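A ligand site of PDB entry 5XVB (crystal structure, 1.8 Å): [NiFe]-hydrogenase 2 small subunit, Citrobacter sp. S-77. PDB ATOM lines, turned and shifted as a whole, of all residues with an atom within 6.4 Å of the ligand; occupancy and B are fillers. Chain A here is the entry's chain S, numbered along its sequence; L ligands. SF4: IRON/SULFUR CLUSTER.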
ATOM      1  N   ILE A 191     -23.799 -26.782 -19.025  1.00  0.00           N
ATOM      2  CA  ILE A 191     -22.915 -26.314 -17.970  1.00  0.00           C
ATOM      3  C   ILE A 191     -22.946 -24.780 -17.926  1.00  0.00           C
ATOM      4  O   ILE A 191     -23.080 -24.174 -16.854  1.00  0.00           O
ATOM      5  CB  ILE A 191     -21.447 -26.840 -18.173  1.00  0.00           C
ATOM      6  CG1 ILE A 191     -21.381 -28.332 -17.853  1.00  0.00           C
ATOM      7  CG2 ILE A 191     -20.455 -26.061 -17.314  1.00  0.00           C
ATOM      8  CD1 ILE A 191     -20.093 -29.033 -18.433  1.00  0.00           C
ATOM      9  N   HIS A 192     -22.909 -24.170 -19.105  1.00  0.00           N
ATOM     10  CA  HIS A 192     -22.951 -22.713 -19.282  1.00  0.00           C
ATOM     11  C   HIS A 192     -24.244 -22.059 -18.776  1.00  0.00           C
ATOM     12  O   HIS A 192     -24.260 -20.863 -18.497  1.00  0.00           O
ATOM     13  CB  HIS A 192     -22.806 -22.416 -20.768  1.00  0.00           C
ATOM     14  CG  HIS A 192     -22.850 -20.970 -21.137  1.00  0.00           C
ATOM     15  ND1 HIS A 192     -21.782 -20.117 -20.945  1.00  0.00           N
ATOM     16  CD2 HIS A 192     -23.815 -20.226 -21.743  1.00  0.00           C
ATOM     17  CE1 HIS A 192     -22.094 -18.903 -21.376  1.00  0.00           C
ATOM     18  NE2 HIS A 192     -23.321 -18.952 -21.868  1.00  0.00           N
ATOM     19  N   GLU A 193     -25.326 -22.826 -18.723  1.00  0.00           N
ATOM     20  CA  GLU A 193     -26.615 -22.323 -18.219  1.00  0.00           C
ATOM     21  C   GLU A 193     -26.729 -22.496 -16.704  1.00  0.00           C
ATOM     22  O   GLU A 193     -27.792 -22.266 -16.103  1.00  0.00           O
ATOM     23  CB  GLU A 193     -27.797 -22.982 -18.929  1.00  0.00           C
ATOM     24  CG  GLU A 193     -27.906 -22.541 -20.404  1.00  0.00           C
ATOM     25  CD  GLU A 193     -28.075 -21.025 -20.521  1.00  0.00           C
ATOM     26  OE1 GLU A 193     -29.031 -20.482 -19.917  1.00  0.00           O
ATOM     27  OE2 GLU A 193     -27.246 -20.371 -21.198  1.00  0.00           O
ATOM     28  N   CYS A 195     -23.399 -21.878 -14.776  1.00  0.00           N
ATOM     29  CA  CYS A 195     -22.001 -21.655 -14.440  1.00  0.00           C
ATOM     30  C   CYS A 195     -21.711 -20.344 -13.715  1.00  0.00           C
ATOM     31  O   CYS A 195     -22.160 -19.266 -14.125  1.00  0.00           O
ATOM     32  CB  CYS A 195     -21.103 -21.777 -15.688  1.00  0.00           C
ATOM     33  SG  CYS A 195     -19.418 -21.376 -15.259  1.00  0.00           S
ATOM     34  N   GLU A 196     -20.921 -20.436 -12.644  1.00  0.00           N
ATOM     35  CA  GLU A 196     -20.715 -19.327 -11.727  1.00  0.00           C
ATOM     36  C   GLU A 196     -19.898 -18.186 -12.330  1.00  0.00           C
ATOM     37  O   GLU A 196     -19.793 -17.122 -11.733  1.00  0.00           O
ATOM     38  CB  GLU A 196     -20.103 -19.829 -10.400  1.00  0.00           C
ATOM     39  CG  GLU A 196     -18.622 -20.278 -10.510  1.00  0.00           C
ATOM     40  CD  GLU A 196     -18.400 -21.769 -10.823  1.00  0.00           C
ATOM     41  OE1 GLU A 196     -19.325 -22.424 -11.379  1.00  0.00           O
ATOM     42  OE2 GLU A 196     -17.278 -22.262 -10.508  1.00  0.00           O
ATOM     43  N   ARG A 197     -19.324 -18.409 -13.516  1.00  0.00           N
ATOM     44  CA  ARG A 197     -18.572 -17.372 -14.195  1.00  0.00           C
ATOM     45  C   ARG A 197     -19.396 -16.654 -15.273  1.00  0.00           C
ATOM     46  O   ARG A 197     -18.930 -15.725 -15.909  1.00  0.00           O
ATOM     47  CB  ARG A 197     -17.251 -17.905 -14.772  1.00  0.00           C
ATOM     48  CG  ARG A 197     -16.350 -18.477 -13.666  1.00  0.00           C
ATOM     49  CD  ARG A 197     -14.995 -18.927 -14.147  1.00  0.00           C
ATOM     50  NE  ARG A 197     -14.225 -19.400 -12.991  1.00  0.00           N
ATOM     51  CZ  ARG A 197     -12.902 -19.365 -12.902  1.00  0.00           C
ATOM     52  NH1 ARG A 197     -12.174 -18.867 -13.911  1.00  0.00           N
ATOM     53  NH2 ARG A 197     -12.296 -19.830 -11.813  1.00  0.00           N
ATOM     54  N   ARG A 198     -20.638 -17.087 -15.459  1.00  0.00           N
ATOM     55  CA  ARG A 198     -21.582 -16.389 -16.328  1.00  0.00           C
ATOM     56  C   ARG A 198     -21.606 -14.850 -16.156  1.00  0.00           C
ATOM     57  O   ARG A 198     -21.620 -14.121 -17.167  1.00  0.00           O
ATOM     58  CB  ARG A 198     -22.980 -17.004 -16.229  1.00  0.00           C
ATOM     59  CG  ARG A 198     -24.023 -16.434 -17.182  1.00  0.00           C
ATOM     60  CD  ARG A 198     -23.652 -16.650 -18.666  1.00  0.00           C
ATOM     61  NE  ARG A 198     -24.750 -16.185 -19.503  1.00  0.00           N
ATOM     62  CZ  ARG A 198     -25.701 -16.969 -20.009  1.00  0.00           C
ATOM     63  NH1 ARG A 198     -25.668 -18.296 -19.799  1.00  0.00           N
ATOM     64  NH2 ARG A 198     -26.681 -16.432 -20.731  1.00  0.00           N
ATOM     65  N   PRO A 199     -21.598 -14.335 -14.908  1.00  0.00           N
ATOM     66  CA  PRO A 199     -21.513 -12.867 -14.808  1.00  0.00           C
ATOM     67  C   PRO A 199     -20.324 -12.235 -15.533  1.00  0.00           C
ATOM     68  O   PRO A 199     -20.425 -11.118 -16.038  1.00  0.00           O
ATOM     69  CB  PRO A 199     -21.357 -12.610 -13.297  1.00  0.00           C
ATOM     70  CG  PRO A 199     -21.974 -13.803 -12.657  1.00  0.00           C
ATOM     71  CD  PRO A 199     -21.653 -14.964 -13.561  1.00  0.00           C
ATOM     72  N   PHE A 201     -18.618 -13.584 -18.223  1.00  0.00           N
ATOM     73  CA  PHE A 201     -19.051 -13.747 -19.630  1.00  0.00           C
ATOM     74  C   PHE A 201     -19.966 -12.601 -20.069  1.00  0.00           C
ATOM     75  O   PHE A 201     -19.768 -12.019 -21.135  1.00  0.00           O
ATOM     76  CB  PHE A 201     -19.807 -15.081 -19.768  1.00  0.00           C
ATOM     77  CG  PHE A 201     -20.320 -15.375 -21.161  1.00  0.00           C
ATOM     78  CD1 PHE A 201     -19.536 -16.069 -22.075  1.00  0.00           C
ATOM     79  CD2 PHE A 201     -21.601 -14.973 -21.549  1.00  0.00           C
ATOM     80  CE1 PHE A 201     -20.014 -16.348 -23.352  1.00  0.00           C
ATOM     81  CE2 PHE A 201     -22.073 -15.255 -22.805  1.00  0.00           C
ATOM     82  CZ  PHE A 201     -21.272 -15.938 -23.722  1.00  0.00           C
ATOM     83  N   PHE A 206     -12.901 -11.687 -19.492  1.00  0.00           N
ATOM     84  CA  PHE A 206     -12.404 -12.967 -19.992  1.00  0.00           C
ATOM     85  C   PHE A 206     -10.931 -13.145 -19.667  1.00  0.00           C
ATOM     86  O   PHE A 206     -10.169 -12.193 -19.718  1.00  0.00           O
ATOM     87  CB  PHE A 206     -12.568 -13.033 -21.510  1.00  0.00           C
ATOM     88  CG  PHE A 206     -13.983 -13.080 -21.959  1.00  0.00           C
ATOM     89  CD1 PHE A 206     -14.776 -14.181 -21.684  1.00  0.00           C
ATOM     90  CD2 PHE A 206     -14.540 -12.035 -22.689  1.00  0.00           C
ATOM     91  CE1 PHE A 206     -16.094 -14.239 -22.107  1.00  0.00           C
ATOM     92  CE2 PHE A 206     -15.860 -12.094 -23.126  1.00  0.00           C
ATOM     93  CZ  PHE A 206     -16.634 -13.182 -22.841  1.00  0.00           C
ATOM     94  N   TRP A 219     -11.937 -14.930 -13.919  1.00  0.00           N
ATOM     95  CA  TRP A 219     -12.900 -14.511 -14.926  1.00  0.00           C
ATOM     96  C   TRP A 219     -13.296 -15.681 -15.844  1.00  0.00           C
ATOM     97  O   TRP A 219     -12.744 -16.776 -15.744  1.00  0.00           O
ATOM     98  CB  TRP A 219     -12.319 -13.368 -15.751  1.00  0.00           C
ATOM     99  CG  TRP A 219     -12.237 -12.071 -15.021  1.00  0.00           C
ATOM    100  CD1 TRP A 219     -12.689 -11.791 -13.747  1.00  0.00           C
ATOM    101  CD2 TRP A 219     -11.692 -10.849 -15.534  1.00  0.00           C
ATOM    102  NE1 TRP A 219     -12.427 -10.476 -13.441  1.00  0.00           N
ATOM    103  CE2 TRP A 219     -11.827  -9.877 -14.515  1.00  0.00           C
ATOM    104  CE3 TRP A 219     -11.102 -10.471 -16.752  1.00  0.00           C
ATOM    105  CZ2 TRP A 219     -11.394  -8.559 -14.679  1.00  0.00           C
ATOM    106  CZ3 TRP A 219     -10.664  -9.158 -16.910  1.00  0.00           C
ATOM    107  CH2 TRP A 219     -10.822  -8.219 -15.870  1.00  0.00           C
ATOM    108  N   CYS A 220     -14.239 -15.427 -16.746  1.00  0.00           N
ATOM    109  CA  CYS A 220     -14.791 -16.446 -17.629  1.00  0.00           C
ATOM    110  C   CYS A 220     -13.738 -17.026 -18.584  1.00  0.00           C
ATOM    111  O   CYS A 220     -12.865 -16.274 -19.046  1.00  0.00           O
ATOM    112  CB  CYS A 220     -15.931 -15.839 -18.431  1.00  0.00           C
ATOM    113  SG  CYS A 220     -16.487 -16.854 -19.792  1.00  0.00           S
ATOM    114  N   LEU A 221     -13.820 -18.322 -18.900  1.00  0.00           N
ATOM    115  CA  LEU A 221     -12.800 -18.967 -19.739  1.00  0.00           C
ATOM    116  C   LEU A 221     -13.252 -19.220 -21.185  1.00  0.00           C
ATOM    117  O   LEU A 221     -12.647 -20.018 -21.925  1.00  0.00           O
ATOM    118  CB  LEU A 221     -12.354 -20.285 -19.093  1.00  0.00           C
ATOM    119  CG  LEU A 221     -12.004 -20.229 -17.596  1.00  0.00           C
ATOM    120  CD1 LEU A 221     -11.499 -21.584 -17.105  1.00  0.00           C
ATOM    121  CD2 LEU A 221     -10.982 -19.133 -17.290  1.00  0.00           C
ATOM    122  N   TYR A 222     -14.335 -18.555 -21.584  1.00  0.00           N
ATOM    123  CA  TYR A 222     -14.884 -18.745 -22.931  1.00  0.00           C
ATOM    124  C   TYR A 222     -13.833 -18.584 -24.029  1.00  0.00           C
ATOM    125  O   TYR A 222     -13.757 -19.408 -24.954  1.00  0.00           O
ATOM    126  CB  TYR A 222     -16.058 -17.791 -23.223  1.00  0.00           C
ATOM    127  CG  TYR A 222     -16.579 -17.988 -24.637  1.00  0.00           C
ATOM    128  CD1 TYR A 222     -17.407 -19.064 -24.946  1.00  0.00           C
ATOM    129  CD2 TYR A 222     -16.207 -17.134 -25.677  1.00  0.00           C
ATOM    130  CE1 TYR A 222     -17.853 -19.287 -26.246  1.00  0.00           C
ATOM    131  CE2 TYR A 222     -16.660 -17.344 -26.963  1.00  0.00           C
ATOM    132  CZ  TYR A 222     -17.489 -18.412 -27.251  1.00  0.00           C
ATOM    133  OH  TYR A 222     -17.931 -18.640 -28.544  1.00  0.00           O
ATOM    134  N   HIS A 223     -13.032 -17.528 -23.944  1.00  0.00           N
ATOM    135  CA  HIS A 223     -12.036 -17.267 -24.971  1.00  0.00           C
ATOM    136  C   HIS A 223     -10.757 -18.108 -24.895  1.00  0.00           C
ATOM    137  O   HIS A 223      -9.915 -18.053 -25.787  1.00  0.00           O
ATOM    138  CB  HIS A 223     -11.727 -15.785 -25.071  1.00  0.00           C
ATOM    139  CG  HIS A 223     -12.811 -15.010 -25.744  1.00  0.00           C
ATOM    140  ND1 HIS A 223     -12.996 -15.022 -27.107  1.00  0.00           N
ATOM    141  CD2 HIS A 223     -13.797 -14.233 -25.242  1.00  0.00           C
ATOM    142  CE1 HIS A 223     -14.042 -14.281 -27.417  1.00  0.00           C
ATOM    143  NE2 HIS A 223     -14.553 -13.793 -26.304  1.00  0.00           N
ATOM    144  N   CYS A 226     -13.557 -22.556 -23.672  1.00  0.00           N
ATOM    145  CA  CYS A 226     -14.514 -23.269 -22.839  1.00  0.00           C
ATOM    146  C   CYS A 226     -15.705 -23.842 -23.619  1.00  0.00           C
ATOM    147  O   CYS A 226     -16.352 -23.148 -24.409  1.00  0.00           O
ATOM    148  CB  CYS A 226     -15.015 -22.400 -21.660  1.00  0.00           C
ATOM    149  SG  CYS A 226     -16.000 -23.344 -20.496  1.00  0.00           S
ATOM    150  N   LYS A 227     -16.001 -25.109 -23.383  1.00  0.00           N
ATOM    151  CA  LYS A 227     -17.024 -25.798 -24.137  1.00  0.00           C
ATOM    152  C   LYS A 227     -18.292 -25.894 -23.327  1.00  0.00           C
ATOM    153  O   LYS A 227     -19.204 -26.625 -23.691  1.00  0.00           O
ATOM    154  CB  LYS A 227     -16.544 -27.183 -24.520  1.00  0.00           C
ATOM    155  CG  LYS A 227     -15.328 -27.165 -25.439  1.00  0.00           C
ATOM    156  CD  LYS A 227     -15.585 -26.277 -26.663  1.00  0.00           C
ATOM    157  CE  LYS A 227     -14.463 -26.443 -27.712  1.00  0.00           C
ATOM    158  NZ  LYS A 227     -13.122 -26.078 -27.161  1.00  0.00           N
ATOM    159  N   GLY A 228     -18.309 -25.192 -22.191  1.00  0.00           N
ATOM    160  CA  GLY A 228     -19.482 -25.077 -21.346  1.00  0.00           C
ATOM    161  C   GLY A 228     -20.730 -24.748 -22.168  1.00  0.00           C
ATOM    162  O   GLY A 228     -21.748 -25.413 -21.982  1.00  0.00           O
ATOM    163  N   PRO A 229     -20.664 -23.750 -23.076  1.00  0.00           N
ATOM    164  CA  PRO A 229     -21.869 -23.401 -23.855  1.00  0.00           C
ATOM    165  C   PRO A 229     -22.495 -24.529 -24.670  1.00  0.00           C
ATOM    166  O   PRO A 229     -23.683 -24.431 -25.008  1.00  0.00           O
ATOM    167  CB  PRO A 229     -21.370 -22.289 -24.775  1.00  0.00           C
ATOM    168  CG  PRO A 229     -20.337 -21.602 -23.971  1.00  0.00           C
ATOM    169  CD  PRO A 229     -19.623 -22.712 -23.225  1.00  0.00           C
ATOM    170  N   TRP A 247     -13.840 -28.216 -10.010  1.00  0.00           N
ATOM    171  CA  TRP A 247     -14.128 -28.682 -11.344  1.00  0.00           C
ATOM    172  C   TRP A 247     -13.162 -27.997 -12.304  1.00  0.00           C
ATOM    173  O   TRP A 247     -12.449 -27.084 -11.882  1.00  0.00           O
ATOM    174  CB  TRP A 247     -15.615 -28.496 -11.725  1.00  0.00           C
ATOM    175  CG  TRP A 247     -16.132 -27.096 -11.904  1.00  0.00           C
ATOM    176  CD1 TRP A 247     -16.285 -26.145 -10.931  1.00  0.00           C
ATOM    177  CD2 TRP A 247     -16.647 -26.528 -13.121  1.00  0.00           C
ATOM    178  NE1 TRP A 247     -16.839 -25.002 -11.477  1.00  0.00           N
ATOM    179  CE2 TRP A 247     -17.079 -25.213 -12.810  1.00  0.00           C
ATOM    180  CE3 TRP A 247     -16.777 -26.989 -14.445  1.00  0.00           C
ATOM    181  CZ2 TRP A 247     -17.643 -24.361 -13.766  1.00  0.00           C
ATOM    182  CZ3 TRP A 247     -17.325 -26.143 -15.402  1.00  0.00           C
ATOM    183  CH2 TRP A 247     -17.757 -24.837 -15.055  1.00  0.00           C
ATOM    184  N   VAL A 249     -13.155 -25.679 -14.691  1.00  0.00           N
ATOM    185  CA  VAL A 249     -13.012 -24.224 -14.796  1.00  0.00           C
ATOM    186  C   VAL A 249     -12.740 -23.521 -13.474  1.00  0.00           C
ATOM    187  O   VAL A 249     -11.995 -22.546 -13.468  1.00  0.00           O
ATOM    188  CB  VAL A 249     -14.056 -23.475 -15.686  1.00  0.00           C
ATOM    189  CG1 VAL A 249     -14.719 -24.382 -16.765  1.00  0.00           C
ATOM    190  CG2 VAL A 249     -14.992 -22.654 -14.872  1.00  0.00           C
ATOM    191  N   PRO A 254     -10.471 -24.255 -19.236  1.00  0.00           N
ATOM    192  CA  PRO A 254     -11.772 -24.362 -19.893  1.00  0.00           C
ATOM    193  C   PRO A 254     -12.335 -25.778 -19.869  1.00  0.00           C
ATOM    194  O   PRO A 254     -11.560 -26.730 -19.888  1.00  0.00           O
ATOM    195  CB  PRO A 254     -11.481 -23.932 -21.351  1.00  0.00           C
ATOM    196  CG  PRO A 254      -9.966 -24.127 -21.538  1.00  0.00           C
ATOM    197  CD  PRO A 254      -9.391 -23.799 -20.148  1.00  0.00           C
ATOM    198  N   CYS A 255     -13.655 -25.912 -19.764  1.00  0.00           N
ATOM    199  CA  CYS A 255     -14.333 -27.142 -20.164  1.00  0.00           C
ATOM    200  C   CYS A 255     -13.922 -27.545 -21.586  1.00  0.00           C
ATOM    201  O   CYS A 255     -13.895 -26.702 -22.483  1.00  0.00           O
ATOM    202  CB  CYS A 255     -15.837 -26.949 -20.129  1.00  0.00           C
ATOM    203  SG  CYS A 255     -16.781 -28.352 -20.689  1.00  0.00           S
HETATM  204 FE1  SF4 L   1     -17.596 -18.868 -19.216  1.00  0.00          FE
HETATM  205 FE2  SF4 L   1     -18.657 -20.690 -17.432  1.00  0.00          FE
HETATM  206 FE3  SF4 L   1     -19.772 -20.321 -19.896  1.00  0.00          FE
HETATM  207 FE4  SF4 L   1     -17.370 -21.690 -19.630  1.00  0.00          FE
HETATM  208  S1  SF4 L   1     -19.340 -22.193 -18.830  1.00  0.00           S
HETATM  209  S2  SF4 L   1     -17.930 -20.094 -21.029  1.00  0.00           S
HETATM  210  S3  SF4 L   1     -16.564 -20.461 -18.038  1.00  0.00           S
HETATM  211  S4  SF4 L   1     -19.571 -18.853 -18.251  1.00  0.00           S
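S4 of the ligand sits close to N of Arg 198 (3.5 Å).
An iron atom (FE1) of the ligand is bound by the side-chain sulfur (SG) of Cys 220, at 2.4 Å.
SG of Cys 195 binds FE2 of the ligand (2.4 Å).
An iron atom (FE4) of the ligand is bound by the side-chain sulfur (SG) of Cys 226 (2.3 Å).
The backbone NH (N) of Leu 221 sits close to a sulfur (S3) of the ligand.
An iron atom (FE3) of the ligand is bound by a ring nitrogen (ND1) of His 192 (2.3 Å).
A ring nitrogen (NE2) of His 192 is in hydrogen-bond range of the guanidinium group (NH1) of Arg 198 (3.2 Å).
The backbone carbonyl oxygen of Trp 219 is in hydrogen-bond range of the guanidinium group of Arg 197, at 2.8 Å.
The backbone carbonyl oxygen of Leu 221 sits at hydrogen-bond distance from the backbone NH of Cys 226.
The side-chain sulfur (SG) of Cys 195 sits close to the backbone NH (N) of Arg 197 (3.4 Å).
The guanidinium group (NH1) of Arg 198 lies within salt-bridge range of the side-chain carboxylate (OE2) of Glu 193, 3.0 Å away.
The backbone NH (N) of Cys 255 sits close to the side-chain sulfur (SG) of Cys 226, at 3.6 Å.
NH2 of Arg 197 sits at hydrogen-bond distance from O of Val 249.
The backbone NH (N) of Gly 228 sits close to the side-chain sulfur (SG) of Cys 226, 3.4 Å away.
C of Arg 197 touches S4 of the ligand, at 3.7 Å.
CB of Tyr 222 touches S2 of the ligand (3.7 Å).
Gly 228 touches the ligand (CA to S1, 3.8 Å).
Pro 229 touches the ligand (CD to S2, 3.8 Å).
Hydrophobic or aromatic side chains that line the ligand: His 192, Tyr 222 and Pro 229.
Ten residues have an atom within 4 Å of the ligand: His 192, Cys 195, Arg 197, Arg 198, Cys 220, Leu 221, Tyr 222, Cys 226, Gly 228 and Pro 229.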
